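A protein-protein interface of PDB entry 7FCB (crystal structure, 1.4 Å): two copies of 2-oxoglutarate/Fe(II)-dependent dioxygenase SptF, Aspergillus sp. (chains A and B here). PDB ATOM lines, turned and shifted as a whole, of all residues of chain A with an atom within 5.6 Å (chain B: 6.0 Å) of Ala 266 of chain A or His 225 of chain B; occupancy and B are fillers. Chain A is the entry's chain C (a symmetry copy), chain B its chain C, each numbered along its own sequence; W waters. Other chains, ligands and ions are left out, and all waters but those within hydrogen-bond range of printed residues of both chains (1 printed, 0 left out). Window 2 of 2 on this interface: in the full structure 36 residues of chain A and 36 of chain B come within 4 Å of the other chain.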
ATOM      1  N   LYS A 257     -13.070 -17.079 -11.356  1.00  0.00           N
ATOM      2  CA  LYS A 257     -14.145 -17.326 -12.312  1.00  0.00           C
ATOM      3  C   LYS A 257     -14.702 -18.729 -12.121  1.00  0.00           C
ATOM      4  O   LYS A 257     -13.999 -19.638 -11.683  1.00  0.00           O
ATOM      5  CB  LYS A 257     -13.591 -17.246 -13.742  1.00  0.00           C
ATOM      6  CG  LYS A 257     -13.200 -15.849 -14.195  1.00  0.00           C
ATOM      7  CD  LYS A 257     -12.745 -15.843 -15.658  1.00  0.00           C
ATOM      8  CE  LYS A 257     -11.404 -16.510 -15.789  1.00  0.00           C
ATOM      9  NZ  LYS A 257     -10.757 -16.274 -17.120  1.00  0.00           N
ATOM     10  N   ALA A 258     -15.967 -18.923 -12.489  1.00  0.00           N
ATOM     11  CA  ALA A 258     -16.527 -20.267 -12.604  1.00  0.00           C
ATOM     12  C   ALA A 258     -16.427 -20.631 -14.074  1.00  0.00           C
ATOM     13  O   ALA A 258     -17.249 -20.201 -14.889  1.00  0.00           O
ATOM     14  CB  ALA A 258     -17.965 -20.323 -12.104  1.00  0.00           C
ATOM     15  N   GLY A 259     -15.395 -21.393 -14.403  1.00  0.00           N
ATOM     16  CA  GLY A 259     -15.055 -21.615 -15.797  1.00  0.00           C
ATOM     17  C   GLY A 259     -14.695 -20.293 -16.445  1.00  0.00           C
ATOM     18  O   GLY A 259     -13.755 -19.599 -16.027  1.00  0.00           O
ATOM     19  N   ASN A 262     -19.134 -16.080 -14.363  1.00  0.00           N
ATOM     20  CA  ASN A 262     -19.010 -15.530 -13.021  1.00  0.00           C
ATOM     21  C   ASN A 262     -19.469 -16.538 -11.984  1.00  0.00           C
ATOM     22  O   ASN A 262     -20.494 -17.211 -12.152  1.00  0.00           O
ATOM     23  CB  ASN A 262     -19.816 -14.236 -12.868  1.00  0.00           C
ATOM     24  CG  ASN A 262     -19.330 -13.139 -13.779  1.00  0.00           C
ATOM     25  OD1 ASN A 262     -18.142 -13.050 -14.083  1.00  0.00           O
ATOM     26  ND2 ASN A 262     -20.251 -12.294 -14.226  1.00  0.00           N
ATOM     27  N   LEU A 263     -18.724 -16.593 -10.878  1.00  0.00           N
ATOM     28  CA  LEU A 263     -19.029 -17.525  -9.805  1.00  0.00           C
ATOM     29  C   LEU A 263     -20.445 -17.321  -9.277  1.00  0.00           C
ATOM     30  O   LEU A 263     -21.177 -18.295  -9.049  1.00  0.00           O
ATOM     31  CB  LEU A 263     -18.008 -17.335  -8.681  1.00  0.00           C
ATOM     32  CG  LEU A 263     -18.199 -18.172  -7.418  1.00  0.00           C
ATOM     33  CD1 LEU A 263     -18.132 -19.659  -7.731  1.00  0.00           C
ATOM     34  CD2 LEU A 263     -17.146 -17.787  -6.382  1.00  0.00           C
ATOM     35  N   GLU A 264     -20.846 -16.058  -9.084  1.00  0.00           N
ATOM     36  CA  GLU A 264     -22.132 -15.749  -8.452  1.00  0.00           C
ATOM     37  C   GLU A 264     -23.314 -16.063  -9.365  1.00  0.00           C
ATOM     38  O   GLU A 264     -24.441 -16.198  -8.879  1.00  0.00           O
ATOM     39  CB  GLU A 264     -22.122 -14.287  -7.981  1.00  0.00           C
ATOM     40  CG  GLU A 264     -22.030 -13.269  -9.111  1.00  0.00           C
ATOM     41  CD  GLU A 264     -20.611 -12.837  -9.470  1.00  0.00           C
ATOM     42  OE1 GLU A 264     -19.664 -13.650  -9.329  1.00  0.00           O
ATOM     43  OE2 GLU A 264     -20.450 -11.708  -9.985  1.00  0.00           O
ATOM     44  N   ASP A 265     -23.075 -16.210 -10.667  1.00  0.00           N
ATOM     45  CA  ASP A 265     -24.089 -16.766 -11.558  1.00  0.00           C
ATOM     46  C   ASP A 265     -24.112 -18.290 -11.454  1.00  0.00           C
ATOM     47  O   ASP A 265     -25.185 -18.896 -11.325  1.00  0.00           O
ATOM     48  CB  ASP A 265     -23.809 -16.316 -12.998  1.00  0.00           C
ATOM     49  CG  ASP A 265     -24.016 -14.827 -13.193  1.00  0.00           C
ATOM     50  OD1 ASP A 265     -25.006 -14.290 -12.647  1.00  0.00           O
ATOM     51  OD2 ASP A 265     -23.175 -14.187 -13.857  1.00  0.00           O
ATOM     52  N   ALA A 266     -22.935 -18.923 -11.441  1.00  0.00           N
ATOM     53  CA  ALA A 266     -22.891 -20.384 -11.415  1.00  0.00           C
ATOM     54  C   ALA A 266     -23.481 -20.960 -10.136  1.00  0.00           C
ATOM     55  O   ALA A 266     -24.020 -22.071 -10.155  1.00  0.00           O
ATOM     56  CB  ALA A 266     -21.456 -20.882 -11.607  1.00  0.00           C
ATOM     57  N   THR A 267     -23.386 -20.242  -9.022  1.00  0.00           N
ATOM     58  CA  THR A 267     -23.932 -20.714  -7.757  1.00  0.00           C
ATOM     59  C   THR A 267     -25.379 -20.306  -7.561  1.00  0.00           C
ATOM     60  O   THR A 267     -25.971 -20.650  -6.531  1.00  0.00           O
ATOM     61  CB  THR A 267     -23.117 -20.166  -6.582  1.00  0.00           C
ATOM     62  OG1 THR A 267     -23.133 -18.730  -6.623  1.00  0.00           O
ATOM     63  CG2 THR A 267     -21.668 -20.645  -6.650  1.00  0.00           C
ATOM     64  N   GLY A 268     -25.942 -19.551  -8.499  1.00  0.00           N
ATOM     65  CA  GLY A 268     -27.300 -19.080  -8.326  1.00  0.00           C
ATOM     66  C   GLY A 268     -27.444 -18.031  -7.256  1.00  0.00           C
ATOM     67  O   GLY A 268     -28.558 -17.781  -6.789  1.00  0.00           O
ATOM     68  N   ASN B  64     -13.401 -24.930 -16.752  1.00  0.00           N
ATOM     69  CA  ASN B  64     -14.345 -25.711 -15.940  1.00  0.00           C
ATOM     70  C   ASN B  64     -14.078 -27.214 -16.040  1.00  0.00           C
ATOM     71  O   ASN B  64     -15.006 -28.024 -15.989  1.00  0.00           O
ATOM     72  CB  ASN B  64     -15.799 -25.368 -16.326  1.00  0.00           C
ATOM     73  CG  ASN B  64     -16.673 -24.959 -15.149  1.00  0.00           C
ATOM     74  OD1 ASN B  64     -16.300 -25.098 -13.992  1.00  0.00           O
ATOM     75  ND2 ASN B  64     -17.834 -24.391 -15.461  1.00  0.00           N
ATOM     76  N   LEU B  67     -15.186 -29.744 -13.255  1.00  0.00           N
ATOM     77  CA  LEU B  67     -16.622 -29.983 -13.274  1.00  0.00           C
ATOM     78  C   LEU B  67     -17.007 -30.911 -14.414  1.00  0.00           C
ATOM     79  O   LEU B  67     -17.857 -31.791 -14.245  1.00  0.00           O
ATOM     80  CB  LEU B  67     -17.345 -28.650 -13.427  1.00  0.00           C
ATOM     81  CG  LEU B  67     -18.872 -28.702 -13.533  1.00  0.00           C
ATOM     82  CD1 LEU B  67     -19.491 -29.152 -12.232  1.00  0.00           C
ATOM     83  CD2 LEU B  67     -19.414 -27.340 -13.941  1.00  0.00           C
ATOM     84  N   SER B 222     -12.278 -20.338  -9.715  1.00  0.00           N
ATOM     85  CA  SER B 222     -12.845 -20.891  -8.502  1.00  0.00           C
ATOM     86  C   SER B 222     -13.487 -22.237  -8.817  1.00  0.00           C
ATOM     87  O   SER B 222     -13.831 -22.535  -9.966  1.00  0.00           O
ATOM     88  CB  SER B 222     -13.931 -19.957  -7.962  1.00  0.00           C
ATOM     89  OG  SER B 222     -14.549 -20.508  -6.797  1.00  0.00           O
ATOM     90  N   HIS B 223     -13.632 -23.053  -7.778  1.00  0.00           N
ATOM     91  CA  HIS B 223     -14.386 -24.293  -7.875  1.00  0.00           C
ATOM     92  C   HIS B 223     -15.527 -24.359  -6.881  1.00  0.00           C
ATOM     93  O   HIS B 223     -16.093 -25.438  -6.673  1.00  0.00           O
ATOM     94  CB  HIS B 223     -13.457 -25.509  -7.801  1.00  0.00           C
ATOM     95  CG  HIS B 223     -12.533 -25.567  -8.966  1.00  0.00           C
ATOM     96  ND1 HIS B 223     -11.417 -24.760  -9.066  1.00  0.00           N
ATOM     97  CD2 HIS B 223     -12.650 -26.204 -10.152  1.00  0.00           C
ATOM     98  CE1 HIS B 223     -10.856 -24.952 -10.247  1.00  0.00           C
ATOM     99  NE2 HIS B 223     -11.579 -25.822 -10.923  1.00  0.00           N
ATOM    100  N   HIS B 224     -15.899 -23.209  -6.308  1.00  0.00           N
ATOM    101  CA  HIS B 224     -16.910 -23.154  -5.259  1.00  0.00           C
ATOM    102  C   HIS B 224     -18.289 -23.555  -5.766  1.00  0.00           C
ATOM    103  O   HIS B 224     -19.135 -23.951  -4.954  1.00  0.00           O
ATOM    104  CB  HIS B 224     -16.895 -21.746  -4.638  1.00  0.00           C
ATOM    105  CG  HIS B 224     -17.952 -21.505  -3.605  1.00  0.00           C
ATOM    106  ND1 HIS B 224     -18.900 -20.511  -3.725  1.00  0.00           N
ATOM    107  CD2 HIS B 224     -18.183 -22.103  -2.413  1.00  0.00           C
ATOM    108  CE1 HIS B 224     -19.688 -20.526  -2.663  1.00  0.00           C
ATOM    109  NE2 HIS B 224     -19.270 -21.481  -1.850  1.00  0.00           N
ATOM    110  N   HIS B 225     -18.515 -23.495  -7.085  1.00  0.00           N
ATOM    111  CA  HIS B 225     -19.773 -23.907  -7.689  1.00  0.00           C
ATOM    112  C   HIS B 225     -19.885 -25.414  -7.905  1.00  0.00           C
ATOM    113  O   HIS B 225     -20.962 -25.876  -8.304  1.00  0.00           O
ATOM    114  CB  HIS B 225     -19.944 -23.190  -9.028  1.00  0.00           C
ATOM    115  CG  HIS B 225     -18.850 -23.481 -10.001  1.00  0.00           C
ATOM    116  ND1 HIS B 225     -17.533 -23.163  -9.750  1.00  0.00           N
ATOM    117  CD2 HIS B 225     -18.877 -24.031 -11.237  1.00  0.00           C
ATOM    118  CE1 HIS B 225     -16.790 -23.538 -10.777  1.00  0.00           C
ATOM    119  NE2 HIS B 225     -17.584 -24.056 -11.700  1.00  0.00           N
ATOM    120  N   LEU B 226     -18.827 -26.191  -7.677  1.00  0.00           N
ATOM    121  CA  LEU B 226     -18.914 -27.621  -7.944  1.00  0.00           C
ATOM    122  C   LEU B 226     -19.820 -28.290  -6.913  1.00  0.00           C
ATOM    123  O   LEU B 226     -19.848 -27.894  -5.748  1.00  0.00           O
ATOM    124  CB  LEU B 226     -17.532 -28.272  -7.894  1.00  0.00           C
ATOM    125  CG  LEU B 226     -16.824 -28.414  -9.247  1.00  0.00           C
ATOM    126  CD1 LEU B 226     -16.607 -27.039  -9.901  1.00  0.00           C
ATOM    127  CD2 LEU B 226     -15.519 -29.179  -9.123  1.00  0.00           C
ATOM    128  N   PRO B 227     -20.577 -29.305  -7.319  1.00  0.00           N
ATOM    129  CA  PRO B 227     -21.423 -30.017  -6.357  1.00  0.00           C
ATOM    130  C   PRO B 227     -20.606 -30.656  -5.245  1.00  0.00           C
ATOM    131  O   PRO B 227     -19.491 -31.139  -5.456  1.00  0.00           O
ATOM    132  CB  PRO B 227     -22.123 -31.082  -7.210  1.00  0.00           C
ATOM    133  CG  PRO B 227     -21.947 -30.690  -8.613  1.00  0.00           C
ATOM    134  CD  PRO B 227     -20.799 -29.729  -8.708  1.00  0.00           C
HETATM  135  O   HOH W   1     -13.826 -23.215 -12.762  1.00  0.00           O
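The backbone NH of Ser 222 of chain B is in hydrogen-bond range of the backbone carbonyl oxygen of Lys 257 of chain A (2.7 Å).
N of His 224 of chain B lies within hydrogen-bond range of OG of Ser 222 of chain B (3.1 Å).
A ring nitrogen (NE2) of His 225 of chain B is in hydrogen-bond range of the side-chain amide oxygen (OD1) of Asn 64 of chain B (2.8 Å).
OG1 of Thr 267 of chain A lies within hydrogen-bond range of O of Leu 263 of chain A (3.1 Å).
CE1 of His 225 of chain B touches CB of Ala 258 of chain A (3.7 Å).
Gly 259 of chain A touches Asn 64 of chain B.
Leu 263 of chain A touches Ser 222 of chain B.
Leu 263 of chain A touches His 224 of chain B.
His 225 of chain B touches Leu 263 of chain A.
Ala 266 of chain A touches His 225 of chain B (CB to CB, 3.8 Å).
CG2 of Thr 267 of chain A touches CB of His 225 of chain B (3.9 Å).
Ala 266 of chain A touches just one residue of chain B: His 225 (3.8 Å).
Printed residues of chain A within 4 Å of Asn 64 of chain B: Gly 259.
Leu 67 of chain B touches none of the printed residues of chain A.
His 223 of chain B touches none of the printed residues of chain A.
Printed residues of chain A within 4 Å of His 224 of chain B: Leu 263 (3.9 Å).
His 225 of chain B touches just these residues of chain A: Ala 258 (3.7 Å), Leu 263 (3.9 Å), Ala 266 (3.8 Å) and Thr 267 (3.9 Å).
Of the 10 printed residues of chain A, 6 touch a printed residue of chain B.
Printed residues of chain A that touch a printed residue of chain B: Lys 257, Ala 258, Gly 259, Leu 263, Ala 266 and Thr 267.
Hydrophobic or aromatic side chains of chain A that line the printed part of chain B: Ala 258, Leu 263 and Ala 266.
Along chain A the printed residues that touch a printed residue of chain B span positions 257 to 267.
Of the 8 printed residues of chain B, 4 touch a printed residue of chain A.
Among the printed residues, 8 pairs touch across the chains.
No position is printed for both chains.
Water W1 lies within hydrogen-bond range of the backbone carbonyl oxygen of Ser 222 of chain B (2.9 Å), the backbone NH of Gly 259 of chain A (2.9 Å) and the side-chain amide oxygen of Asn 64 of chain B (3.3 Å).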
